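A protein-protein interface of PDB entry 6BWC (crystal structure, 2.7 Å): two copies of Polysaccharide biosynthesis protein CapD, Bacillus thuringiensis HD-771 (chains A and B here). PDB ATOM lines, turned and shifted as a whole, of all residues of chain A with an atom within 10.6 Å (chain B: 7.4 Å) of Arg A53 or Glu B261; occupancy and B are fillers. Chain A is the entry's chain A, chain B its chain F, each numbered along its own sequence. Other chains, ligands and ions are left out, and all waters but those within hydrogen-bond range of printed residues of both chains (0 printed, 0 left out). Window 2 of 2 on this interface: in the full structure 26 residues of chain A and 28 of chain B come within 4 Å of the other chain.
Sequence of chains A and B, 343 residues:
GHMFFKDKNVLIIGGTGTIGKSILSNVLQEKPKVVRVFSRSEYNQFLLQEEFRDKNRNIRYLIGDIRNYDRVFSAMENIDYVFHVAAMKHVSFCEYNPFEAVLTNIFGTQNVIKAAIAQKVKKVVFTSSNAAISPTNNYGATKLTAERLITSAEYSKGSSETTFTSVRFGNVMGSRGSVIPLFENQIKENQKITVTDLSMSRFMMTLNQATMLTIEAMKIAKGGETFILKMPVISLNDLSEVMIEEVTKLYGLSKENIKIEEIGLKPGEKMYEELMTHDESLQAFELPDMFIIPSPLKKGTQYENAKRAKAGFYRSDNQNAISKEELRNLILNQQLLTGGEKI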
ATOM      1  N   LEU A  24     -42.042 -27.807  -0.938  1.00  0.00           N
ATOM      2  CA  LEU A  24     -40.973 -28.790  -0.863  1.00  0.00           C
ATOM      3  C   LEU A  24     -41.176 -29.661   0.353  1.00  0.00           C
ATOM      4  O   LEU A  24     -41.372 -30.869   0.227  1.00  0.00           O
ATOM      5  CB  LEU A  24     -39.595 -28.100  -0.845  1.00  0.00           C
ATOM      6  CG  LEU A  24     -38.343 -28.897  -0.494  1.00  0.00           C
ATOM      7  CD1 LEU A  24     -38.091 -29.991  -1.499  1.00  0.00           C
ATOM      8  CD2 LEU A  24     -37.152 -27.972  -0.409  1.00  0.00           C
ATOM      9  N   LEU A  28     -42.290 -33.567   0.926  1.00  0.00           N
ATOM     10  CA  LEU A  28     -41.373 -34.502   1.549  1.00  0.00           C
ATOM     11  C   LEU A  28     -41.984 -35.309   2.673  1.00  0.00           C
ATOM     12  O   LEU A  28     -41.553 -36.423   2.902  1.00  0.00           O
ATOM     13  CB  LEU A  28     -40.155 -33.783   2.116  1.00  0.00           C
ATOM     14  CG  LEU A  28     -39.081 -33.277   1.174  1.00  0.00           C
ATOM     15  CD1 LEU A  28     -38.019 -32.593   2.010  1.00  0.00           C
ATOM     16  CD2 LEU A  28     -38.483 -34.414   0.369  1.00  0.00           C
ATOM     17  N   GLN A  45     -29.666 -21.937  -3.375  1.00  0.00           N
ATOM     18  CA  GLN A  45     -29.596 -23.403  -3.288  1.00  0.00           C
ATOM     19  C   GLN A  45     -28.654 -23.847  -2.179  1.00  0.00           C
ATOM     20  O   GLN A  45     -28.875 -24.881  -1.569  1.00  0.00           O
ATOM     21  CB  GLN A  45     -29.166 -24.037  -4.603  1.00  0.00           C
ATOM     22  CG  GLN A  45     -30.268 -23.972  -5.641  1.00  0.00           C
ATOM     23  CD  GLN A  45     -30.155 -24.983  -6.753  1.00  0.00           C
ATOM     24  OE1 GLN A  45     -29.238 -25.778  -6.813  1.00  0.00           O
ATOM     25  NE2 GLN A  45     -31.103 -24.932  -7.656  1.00  0.00           N
ATOM     26  N   PHE A  46     -27.615 -23.050  -1.939  1.00  0.00           N
ATOM     27  CA  PHE A  46     -26.586 -23.352  -0.936  1.00  0.00           C
ATOM     28  C   PHE A  46     -27.218 -23.340   0.457  1.00  0.00           C
ATOM     29  O   PHE A  46     -27.151 -24.339   1.170  1.00  0.00           O
ATOM     30  CB  PHE A  46     -25.389 -22.355  -1.072  1.00  0.00           C
ATOM     31  CG  PHE A  46     -24.304 -22.526  -0.030  1.00  0.00           C
ATOM     32  CD1 PHE A  46     -23.396 -23.603  -0.105  1.00  0.00           C
ATOM     33  CD2 PHE A  46     -24.180 -21.615   1.025  1.00  0.00           C
ATOM     34  CE1 PHE A  46     -22.400 -23.760   0.851  1.00  0.00           C
ATOM     35  CE2 PHE A  46     -23.191 -21.776   1.986  1.00  0.00           C
ATOM     36  CZ  PHE A  46     -22.301 -22.843   1.897  1.00  0.00           C
ATOM     37  N   LEU A  47     -27.842 -22.215   0.808  1.00  0.00           N
ATOM     38  CA  LEU A  47     -28.467 -22.030   2.125  1.00  0.00           C
ATOM     39  C   LEU A  47     -29.522 -23.098   2.428  1.00  0.00           C
ATOM     40  O   LEU A  47     -29.589 -23.595   3.554  1.00  0.00           O
ATOM     41  CB  LEU A  47     -29.136 -20.654   2.225  1.00  0.00           C
ATOM     42  CG  LEU A  47     -28.284 -19.383   2.214  1.00  0.00           C
ATOM     43  CD1 LEU A  47     -29.213 -18.171   2.145  1.00  0.00           C
ATOM     44  CD2 LEU A  47     -27.346 -19.310   3.424  1.00  0.00           C
ATOM     45  N   LEU A  48     -30.337 -23.409   1.414  1.00  0.00           N
ATOM     46  CA  LEU A  48     -31.375 -24.442   1.450  1.00  0.00           C
ATOM     47  C   LEU A  48     -30.785 -25.837   1.579  1.00  0.00           C
ATOM     48  O   LEU A  48     -31.291 -26.662   2.326  1.00  0.00           O
ATOM     49  CB  LEU A  48     -32.229 -24.377   0.164  1.00  0.00           C
ATOM     50  CG  LEU A  48     -33.378 -25.388   0.023  1.00  0.00           C
ATOM     51  CD1 LEU A  48     -34.257 -25.390   1.264  1.00  0.00           C
ATOM     52  CD2 LEU A  48     -34.219 -25.109  -1.216  1.00  0.00           C
ATOM     53  N   GLN A  49     -29.723 -26.090   0.825  1.00  0.00           N
ATOM     54  CA  GLN A  49     -28.910 -27.299   0.976  1.00  0.00           C
ATOM     55  C   GLN A  49     -28.471 -27.553   2.410  1.00  0.00           C
ATOM     56  O   GLN A  49     -28.431 -28.698   2.868  1.00  0.00           O
ATOM     57  CB  GLN A  49     -27.648 -27.167   0.144  1.00  0.00           C
ATOM     58  CG  GLN A  49     -27.259 -28.401  -0.638  1.00  0.00           C
ATOM     59  CD  GLN A  49     -26.428 -28.022  -1.840  1.00  0.00           C
ATOM     60  OE1 GLN A  49     -26.722 -28.451  -2.955  1.00  0.00           O
ATOM     61  NE2 GLN A  49     -25.404 -27.185  -1.629  1.00  0.00           N
ATOM     62  N   GLU A  50     -28.104 -26.467   3.090  1.00  0.00           N
ATOM     63  CA  GLU A  50     -27.648 -26.508   4.479  1.00  0.00           C
ATOM     64  C   GLU A  50     -28.775 -26.714   5.480  1.00  0.00           C
ATOM     65  O   GLU A  50     -28.574 -27.296   6.536  1.00  0.00           O
ATOM     66  CB  GLU A  50     -26.877 -25.231   4.828  1.00  0.00           C
ATOM     67  CG  GLU A  50     -25.723 -25.503   5.776  1.00  0.00           C
ATOM     68  CD  GLU A  50     -24.712 -26.455   5.150  1.00  0.00           C
ATOM     69  OE1 GLU A  50     -24.167 -26.141   4.058  1.00  0.00           O
ATOM     70  OE2 GLU A  50     -24.501 -27.535   5.740  1.00  0.00           O
ATOM     71  N   GLU A  51     -29.949 -26.214   5.124  1.00  0.00           N
ATOM     72  CA  GLU A  51     -31.159 -26.324   5.910  1.00  0.00           C
ATOM     73  C   GLU A  51     -31.858 -27.706   5.753  1.00  0.00           C
ATOM     74  O   GLU A  51     -32.843 -27.967   6.448  1.00  0.00           O
ATOM     75  CB  GLU A  51     -32.081 -25.186   5.463  1.00  0.00           C
ATOM     76  CG  GLU A  51     -33.279 -24.867   6.332  1.00  0.00           C
ATOM     77  CD  GLU A  51     -33.936 -23.545   5.926  1.00  0.00           C
ATOM     78  OE1 GLU A  51     -33.943 -23.208   4.714  1.00  0.00           O
ATOM     79  OE2 GLU A  51     -34.438 -22.823   6.819  1.00  0.00           O
ATOM     80  N   PHE A  52     -31.384 -28.562   4.834  1.00  0.00           N
ATOM     81  CA  PHE A  52     -31.943 -29.913   4.599  1.00  0.00           C
ATOM     82  C   PHE A  52     -30.803 -30.907   4.638  1.00  0.00           C
ATOM     83  O   PHE A  52     -30.717 -31.845   3.827  1.00  0.00           O
ATOM     84  CB  PHE A  52     -32.672 -29.984   3.250  1.00  0.00           C
ATOM     85  CG  PHE A  52     -34.066 -29.445   3.297  1.00  0.00           C
ATOM     86  CD1 PHE A  52     -34.284 -28.079   3.393  1.00  0.00           C
ATOM     87  CD2 PHE A  52     -35.156 -30.287   3.266  1.00  0.00           C
ATOM     88  CE1 PHE A  52     -35.565 -27.558   3.452  1.00  0.00           C
ATOM     89  CE2 PHE A  52     -36.440 -29.775   3.324  1.00  0.00           C
ATOM     90  CZ  PHE A  52     -36.649 -28.414   3.411  1.00  0.00           C
ATOM     91  N   ARG A  53     -29.942 -30.703   5.626  1.00  0.00           N
ATOM     92  CA  ARG A  53     -28.692 -31.427   5.719  1.00  0.00           C
ATOM     93  C   ARG A  53     -28.848 -32.872   6.214  1.00  0.00           C
ATOM     94  O   ARG A  53     -27.852 -33.594   6.272  1.00  0.00           O
ATOM     95  CB  ARG A  53     -27.724 -30.678   6.631  1.00  0.00           C
ATOM     96  CG  ARG A  53     -26.270 -30.986   6.339  1.00  0.00           C
ATOM     97  CD  ARG A  53     -25.345 -30.613   7.486  1.00  0.00           C
ATOM     98  NE  ARG A  53     -24.184 -31.501   7.525  1.00  0.00           N
ATOM     99  CZ  ARG A  53     -23.197 -31.521   6.626  1.00  0.00           C
ATOM    100  NH1 ARG A  53     -23.190 -30.701   5.570  1.00  0.00           N
ATOM    101  NH2 ARG A  53     -22.196 -32.381   6.788  1.00  0.00           N
ATOM    102  N   ASP A  54     -30.061 -33.289   6.597  1.00  0.00           N
ATOM    103  CA  ASP A  54     -30.326 -34.697   6.945  1.00  0.00           C
ATOM    104  C   ASP A  54     -31.538 -35.364   6.257  1.00  0.00           C
ATOM    105  O   ASP A  54     -31.746 -36.581   6.387  1.00  0.00           O
ATOM    106  CB  ASP A  54     -30.416 -34.796   8.468  1.00  0.00           C
ATOM    107  CG  ASP A  54     -29.058 -34.565   9.136  1.00  0.00           C
ATOM    108  OD1 ASP A  54     -28.630 -33.392   9.287  1.00  0.00           O
ATOM    109  OD2 ASP A  54     -28.396 -35.569   9.472  1.00  0.00           O
ATOM    110  N   LYS A  55     -32.255 -34.588   5.442  1.00  0.00           N
ATOM    111  CA  LYS A  55     -33.660 -34.843   5.133  1.00  0.00           C
ATOM    112  C   LYS A  55     -33.936 -34.774   3.625  1.00  0.00           C
ATOM    113  O   LYS A  55     -33.552 -35.664   2.862  1.00  0.00           O
ATOM    114  CB  LYS A  55     -34.534 -33.812   5.884  1.00  0.00           C
ATOM    115  CG  LYS A  55     -33.845 -33.125   7.083  1.00  0.00           C
ATOM    116  CD  LYS A  55     -34.744 -32.113   7.799  1.00  0.00           C
ATOM    117  CE  LYS A  55     -33.976 -31.181   8.737  1.00  0.00           C
ATOM    118  NZ  LYS A  55     -34.827 -30.038   9.164  1.00  0.00           N
ATOM    119  N   ASN A  58     -32.123 -37.855  -0.984  1.00  0.00           N
ATOM    120  CA  ASN A  58     -33.551 -37.697  -1.320  1.00  0.00           C
ATOM    121  C   ASN A  58     -33.981 -36.386  -2.043  1.00  0.00           C
ATOM    122  O   ASN A  58     -35.127 -36.271  -2.496  1.00  0.00           O
ATOM    123  CB  ASN A  58     -34.362 -37.811  -0.032  1.00  0.00           C
ATOM    124  CG  ASN A  58     -35.822 -38.107  -0.290  1.00  0.00           C
ATOM    125  OD1 ASN A  58     -36.169 -39.197  -0.741  1.00  0.00           O
ATOM    126  ND2 ASN A  58     -36.685 -37.136  -0.017  1.00  0.00           N
ATOM    127  N   ILE A  59     -33.079 -35.404  -2.120  1.00  0.00           N
ATOM    128  CA  ILE A  59     -33.353 -34.087  -2.711  1.00  0.00           C
ATOM    129  C   ILE A  59     -32.222 -33.727  -3.653  1.00  0.00           C
ATOM    130  O   ILE A  59     -31.150 -33.355  -3.190  1.00  0.00           O
ATOM    131  CB  ILE A  59     -33.419 -32.977  -1.627  1.00  0.00           C
ATOM    132  CG1 ILE A  59     -34.497 -33.289  -0.602  1.00  0.00           C
ATOM    133  CG2 ILE A  59     -33.680 -31.605  -2.240  1.00  0.00           C
ATOM    134  CD1 ILE A  59     -34.427 -32.386   0.612  1.00  0.00           C
ATOM    135  N   TYR A  61     -30.516 -31.000  -6.221  1.00  0.00           N
ATOM    136  CA  TYR A  61     -30.536 -29.547  -6.428  1.00  0.00           C
ATOM    137  C   TYR A  61     -29.975 -29.241  -7.802  1.00  0.00           C
ATOM    138  O   TYR A  61     -28.823 -29.505  -8.050  1.00  0.00           O
ATOM    139  CB  TYR A  61     -29.727 -28.815  -5.329  1.00  0.00           C
ATOM    140  CG  TYR A  61     -30.265 -29.002  -3.910  1.00  0.00           C
ATOM    141  CD1 TYR A  61     -31.188 -28.093  -3.342  1.00  0.00           C
ATOM    142  CD2 TYR A  61     -29.869 -30.100  -3.147  1.00  0.00           C
ATOM    143  CE1 TYR A  61     -31.695 -28.283  -2.051  1.00  0.00           C
ATOM    144  CE2 TYR A  61     -30.358 -30.303  -1.858  1.00  0.00           C
ATOM    145  CZ  TYR A  61     -31.269 -29.404  -1.305  1.00  0.00           C
ATOM    146  OH  TYR A  61     -31.725 -29.668  -0.029  1.00  0.00           O
ATOM    147  N   LEU B 182     -21.041 -19.519   7.184  1.00  0.00           N
ATOM    148  CA  LEU B 182     -21.509 -20.891   7.395  1.00  0.00           C
ATOM    149  C   LEU B 182     -21.275 -21.373   8.851  1.00  0.00           C
ATOM    150  O   LEU B 182     -22.247 -21.541   9.628  1.00  0.00           O
ATOM    151  CB  LEU B 182     -20.859 -21.828   6.377  1.00  0.00           C
ATOM    152  CG  LEU B 182     -21.148 -23.320   6.470  1.00  0.00           C
ATOM    153  CD1 LEU B 182     -22.611 -23.559   6.161  1.00  0.00           C
ATOM    154  CD2 LEU B 182     -20.240 -24.108   5.531  1.00  0.00           C
ATOM    155  N   PHE B 183     -20.002 -21.556   9.222  1.00  0.00           N
ATOM    156  CA  PHE B 183     -19.634 -21.929  10.590  1.00  0.00           C
ATOM    157  C   PHE B 183     -20.316 -21.090  11.658  1.00  0.00           C
ATOM    158  O   PHE B 183     -20.648 -21.619  12.704  1.00  0.00           O
ATOM    159  CB  PHE B 183     -18.134 -21.774  10.814  1.00  0.00           C
ATOM    160  CG  PHE B 183     -17.284 -22.772  10.096  1.00  0.00           C
ATOM    161  CD1 PHE B 183     -17.821 -23.877   9.463  1.00  0.00           C
ATOM    162  CD2 PHE B 183     -15.907 -22.602  10.083  1.00  0.00           C
ATOM    163  CE1 PHE B 183     -17.002 -24.782   8.843  1.00  0.00           C
ATOM    164  CE2 PHE B 183     -15.076 -23.513   9.446  1.00  0.00           C
ATOM    165  CZ  PHE B 183     -15.626 -24.606   8.829  1.00  0.00           C
ATOM    166  N   GLN B 186     -23.876 -22.235  11.566  1.00  0.00           N
ATOM    167  CA  GLN B 186     -23.942 -23.658  11.913  1.00  0.00           C
ATOM    168  C   GLN B 186     -23.853 -23.882  13.423  1.00  0.00           C
ATOM    169  O   GLN B 186     -24.589 -24.672  13.975  1.00  0.00           O
ATOM    170  CB  GLN B 186     -22.847 -24.449  11.191  1.00  0.00           C
ATOM    171  CG  GLN B 186     -23.089 -24.733   9.715  1.00  0.00           C
ATOM    172  CD  GLN B 186     -22.083 -25.727   9.152  1.00  0.00           C
ATOM    173  OE1 GLN B 186     -20.987 -25.894   9.686  1.00  0.00           O
ATOM    174  NE2 GLN B 186     -22.452 -26.391   8.069  1.00  0.00           N
ATOM    175  N   ASN B 190     -27.081 -25.387  14.981  1.00  0.00           N
ATOM    176  CA  ASN B 190     -26.905 -26.832  15.186  1.00  0.00           C
ATOM    177  C   ASN B 190     -25.728 -27.250  16.049  1.00  0.00           C
ATOM    178  O   ASN B 190     -25.448 -28.451  16.158  1.00  0.00           O
ATOM    179  CB  ASN B 190     -26.797 -27.509  13.823  1.00  0.00           C
ATOM    180  CG  ASN B 190     -27.879 -27.041  12.886  1.00  0.00           C
ATOM    181  OD1 ASN B 190     -29.053 -27.237  13.155  1.00  0.00           O
ATOM    182  ND2 ASN B 190     -27.497 -26.372  11.817  1.00  0.00           N
ATOM    183  N   LYS B 192     -22.840 -27.439  15.413  1.00  0.00           N
ATOM    184  CA  LYS B 192     -22.067 -28.360  14.589  1.00  0.00           C
ATOM    185  C   LYS B 192     -21.280 -27.511  13.598  1.00  0.00           C
ATOM    186  O   LYS B 192     -21.731 -26.447  13.189  1.00  0.00           O
ATOM    187  CB  LYS B 192     -22.984 -29.365  13.865  1.00  0.00           C
ATOM    188  CG  LYS B 192     -22.279 -30.655  13.433  1.00  0.00           C
ATOM    189  CD  LYS B 192     -23.254 -31.745  13.009  1.00  0.00           C
ATOM    190  CE  LYS B 192     -23.844 -32.465  14.216  1.00  0.00           C
ATOM    191  NZ  LYS B 192     -25.048 -33.280  13.877  1.00  0.00           N
ATOM    192  N   ILE B 193     -20.080 -27.971  13.278  1.00  0.00           N
ATOM    193  CA  ILE B 193     -19.255 -27.403  12.221  1.00  0.00           C
ATOM    194  C   ILE B 193     -19.219 -28.504  11.130  1.00  0.00           C
ATOM    195  O   ILE B 193     -19.135 -29.696  11.456  1.00  0.00           O
ATOM    196  CB  ILE B 193     -17.842 -26.986  12.803  1.00  0.00           C
ATOM    197  CG1 ILE B 193     -17.493 -25.532  12.487  1.00  0.00           C
ATOM    198  CG2 ILE B 193     -16.672 -27.862  12.338  1.00  0.00           C
ATOM    199  CD1 ILE B 193     -18.467 -24.513  13.046  1.00  0.00           C
ATOM    200  N   THR B 194     -19.316 -28.123   9.856  1.00  0.00           N
ATOM    201  CA  THR B 194     -19.025 -29.047   8.760  1.00  0.00           C
ATOM    202  C   THR B 194     -17.604 -28.762   8.336  1.00  0.00           C
ATOM    203  O   THR B 194     -17.340 -27.682   7.828  1.00  0.00           O
ATOM    204  CB  THR B 194     -19.909 -28.788   7.526  1.00  0.00           C
ATOM    205  OG1 THR B 194     -21.239 -28.456   7.919  1.00  0.00           O
ATOM    206  CG2 THR B 194     -19.928 -29.995   6.648  1.00  0.00           C
ATOM    207  N   VAL B 195     -16.685 -29.704   8.525  1.00  0.00           N
ATOM    208  CA  VAL B 195     -15.264 -29.489   8.169  1.00  0.00           C
ATOM    209  C   VAL B 195     -14.905 -30.416   7.016  1.00  0.00           C
ATOM    210  O   VAL B 195     -15.243 -31.592   7.051  1.00  0.00           O
ATOM    211  CB  VAL B 195     -14.357 -29.696   9.410  1.00  0.00           C
ATOM    212  CG1 VAL B 195     -13.070 -30.444   9.088  1.00  0.00           C
ATOM    213  CG2 VAL B 195     -14.041 -28.362  10.061  1.00  0.00           C
ATOM    214  N   THR B 196     -14.219 -29.892   6.004  1.00  0.00           N
ATOM    215  CA  THR B 196     -13.838 -30.697   4.826  1.00  0.00           C
ATOM    216  C   THR B 196     -12.503 -31.458   5.062  1.00  0.00           C
ATOM    217  O   THR B 196     -12.498 -32.673   5.346  1.00  0.00           O
ATOM    218  CB  THR B 196     -13.810 -29.837   3.536  1.00  0.00           C
ATOM    219  OG1 THR B 196     -13.061 -28.642   3.765  1.00  0.00           O
ATOM    220  CG2 THR B 196     -15.228 -29.451   3.129  1.00  0.00           C
ATOM    221  N   LEU B 198      -9.041 -30.308   7.235  1.00  0.00           N
ATOM    222  CA  LEU B 198      -8.491 -29.204   8.038  1.00  0.00           C
ATOM    223  C   LEU B 198      -7.116 -28.730   7.575  1.00  0.00           C
ATOM    224  O   LEU B 198      -6.791 -27.555   7.805  1.00  0.00           O
ATOM    225  CB  LEU B 198      -8.465 -29.543   9.536  1.00  0.00           C
ATOM    226  CG  LEU B 198      -9.852 -29.677  10.185  1.00  0.00           C
ATOM    227  CD1 LEU B 198      -9.755 -30.260  11.596  1.00  0.00           C
ATOM    228  CD2 LEU B 198     -10.625 -28.351  10.194  1.00  0.00           C
ATOM    229  N   ILE B 258     -18.878 -28.151  21.273  1.00  0.00           N
ATOM    230  CA  ILE B 258     -19.412 -28.066  19.900  1.00  0.00           C
ATOM    231  C   ILE B 258     -18.832 -29.180  19.001  1.00  0.00           C
ATOM    232  O   ILE B 258     -17.608 -29.363  18.917  1.00  0.00           O
ATOM    233  CB  ILE B 258     -19.135 -26.651  19.303  1.00  0.00           C
ATOM    234  CG1 ILE B 258     -20.204 -25.656  19.775  1.00  0.00           C
ATOM    235  CG2 ILE B 258     -19.096 -26.643  17.774  1.00  0.00           C
ATOM    236  CD1 ILE B 258     -19.679 -24.241  19.901  1.00  0.00           C
ATOM    237  N   LYS B 259     -19.737 -29.887  18.318  1.00  0.00           N
ATOM    238  CA  LYS B 259     -19.391 -31.022  17.462  1.00  0.00           C
ATOM    239  C   LYS B 259     -18.669 -30.571  16.193  1.00  0.00           C
ATOM    240  O   LYS B 259     -19.092 -29.596  15.566  1.00  0.00           O
ATOM    241  CB  LYS B 259     -20.657 -31.803  17.061  1.00  0.00           C
ATOM    242  CG  LYS B 259     -21.283 -32.649  18.170  1.00  0.00           C
ATOM    243  CD  LYS B 259     -22.004 -33.876  17.604  1.00  0.00           C
ATOM    244  CE  LYS B 259     -22.371 -34.879  18.686  1.00  0.00           C
ATOM    245  NZ  LYS B 259     -23.234 -35.970  18.153  1.00  0.00           N
ATOM    246  N   ILE B 260     -17.607 -31.304  15.819  1.00  0.00           N
ATOM    247  CA  ILE B 260     -16.836 -31.084  14.568  1.00  0.00           C
ATOM    248  C   ILE B 260     -16.950 -32.284  13.616  1.00  0.00           C
ATOM    249  O   ILE B 260     -16.167 -33.231  13.688  1.00  0.00           O
ATOM    250  CB  ILE B 260     -15.344 -30.743  14.866  1.00  0.00           C
ATOM    251  CG1 ILE B 260     -15.267 -29.355  15.519  1.00  0.00           C
ATOM    252  CG2 ILE B 260     -14.463 -30.795  13.602  1.00  0.00           C
ATOM    253  CD1 ILE B 260     -13.871 -28.932  15.915  1.00  0.00           C
ATOM    254  N   GLU B 261     -17.933 -32.222  12.720  1.00  0.00           N
ATOM    255  CA  GLU B 261     -18.167 -33.282  11.736  1.00  0.00           C
ATOM    256  C   GLU B 261     -17.182 -33.121  10.576  1.00  0.00           C
ATOM    257  O   GLU B 261     -16.840 -32.004  10.170  1.00  0.00           O
ATOM    258  CB  GLU B 261     -19.632 -33.263  11.224  1.00  0.00           C
ATOM    259  CG  GLU B 261     -20.048 -34.462  10.358  1.00  0.00           C
ATOM    260  CD  GLU B 261     -21.426 -34.324   9.714  1.00  0.00           C
ATOM    261  OE1 GLU B 261     -22.336 -33.674  10.290  1.00  0.00           O
ATOM    262  OE2 GLU B 261     -21.604 -34.879   8.608  1.00  0.00           O
ATOM    263  N   GLU B 262     -16.739 -34.259  10.057  1.00  0.00           N
ATOM    264  CA  GLU B 262     -15.878 -34.321   8.901  1.00  0.00           C
ATOM    265  C   GLU B 262     -16.716 -34.744   7.685  1.00  0.00           C
ATOM    266  O   GLU B 262     -16.805 -35.937   7.415  1.00  0.00           O
ATOM    267  CB  GLU B 262     -14.759 -35.325   9.194  1.00  0.00           C
ATOM    268  CG  GLU B 262     -13.771 -35.564   8.056  1.00  0.00           C
ATOM    269  CD  GLU B 262     -12.317 -35.541   8.505  1.00  0.00           C
ATOM    270  OE1 GLU B 262     -12.024 -35.948   9.655  1.00  0.00           O
ATOM    271  OE2 GLU B 262     -11.462 -35.112   7.697  1.00  0.00           O
ATOM    272  N   ILE B 263     -17.339 -33.793   6.965  1.00  0.00           N
ATOM    273  CA  ILE B 263     -18.018 -34.097   5.663  1.00  0.00           C
ATOM    274  C   ILE B 263     -17.032 -34.686   4.642  1.00  0.00           C
ATOM    275  O   ILE B 263     -17.372 -35.619   3.912  1.00  0.00           O
ATOM    276  CB  ILE B 263     -18.794 -32.880   5.030  1.00  0.00           C
ATOM    277  CG1 ILE B 263     -19.784 -33.365   3.922  1.00  0.00           C
ATOM    278  CG2 ILE B 263     -17.848 -31.804   4.479  1.00  0.00           C
ATOM    279  CD1 ILE B 263     -20.531 -32.283   3.136  1.00  0.00           C
ATOM    280  N   GLY B 264     -15.809 -34.162   4.644  1.00  0.00           N
ATOM    281  CA  GLY B 264     -14.757 -34.582   3.734  1.00  0.00           C
ATOM    282  C   GLY B 264     -14.706 -33.628   2.563  1.00  0.00           C
ATOM    283  O   GLY B 264     -15.535 -32.733   2.451  1.00  0.00           O
ATOM    284  N   LYS B 266     -15.383 -31.717  -0.647  1.00  0.00           N
ATOM    285  CA  LYS B 266     -16.378 -31.544  -1.694  1.00  0.00           C
ATOM    286  C   LYS B 266     -15.673 -31.760  -3.044  1.00  0.00           C
ATOM    287  O   LYS B 266     -14.451 -31.540  -3.159  1.00  0.00           O
ATOM    288  CB  LYS B 266     -17.044 -30.164  -1.636  1.00  0.00           C
ATOM    289  CG  LYS B 266     -17.853 -29.914  -0.372  1.00  0.00           C
ATOM    290  CD  LYS B 266     -18.790 -28.715  -0.505  1.00  0.00           C
ATOM    291  CE  LYS B 266     -19.761 -28.661   0.665  1.00  0.00           C
ATOM    292  NZ  LYS B 266     -19.798 -27.315   1.302  1.00  0.00           N
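The side-chain carboxylate (OE2) of Glu B261 is in salt-bridge range of the guanidinium group (NH2) of Arg A53, 3.1 Å away. OE2 of Glu A50 is in hydrogen-bond range of NE2 of Gln B186, at 3.3 Å.
O of Val B195 lies within hydrogen-bond range of N of Ile B263 (3.0 Å). The backbone carbonyl oxygen (O) of Glu B261 sits at hydrogen-bond distance from the backbone NH (N) of Val B195. OE2 of Glu A50 lies within salt-bridge range of NH1 of Arg A53, 3.4 Å away. The backbone NH (N) of Glu B261 sits at hydrogen-bond distance from the backbone carbonyl oxygen (O) of Ile B193 (3.1 Å). N of Thr B194 lies within hydrogen-bond range of OE1 of Gln B186, at 2.8 Å.
Among the printed residues, merely in contact across the chains: Arg A53 with Thr B194, Glu A50 with Leu B182 and Arg A53 with Ile B263.
Of the printed residues of chain B, Glu A50 touches Leu B182 (3.7 Å) and Gln B186 (3.3 Å). Arg A53 touches just these residues of chain B: Thr B194 (3.3 Å), Glu B261 (3.1 Å) and Ile B263 (3.9 Å). Ile A59 touches none of the printed residues of chain B. Of the printed residues of chain A, Leu B182 touches Glu A50. Of chain A, only Arg A53 comes within 4 Å of Thr B194. No residue of chain A comes within 4 Å of Val B195. No residue of chain A comes within 4 Å of Ile B260. Of chain A, only Arg A53 comes within 4 Å of Glu B261. The nearest residue of chain A that does not touch Glu B261 is Asp A54 (6.4 Å). The nearest printed residue of chain A that does not touch Gln B186 is Arg A53 (5.0 Å).
Printed residues of chain A that touch a printed residue of chain B: Glu A50 and Arg A53. Of the 18 printed residues of chain B, 5 touch a printed residue of chain A. Hydrophobic or aromatic side chains of chain B that line the printed part of chain A: Leu B182 and Ile B263.
No position is printed for both chains.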
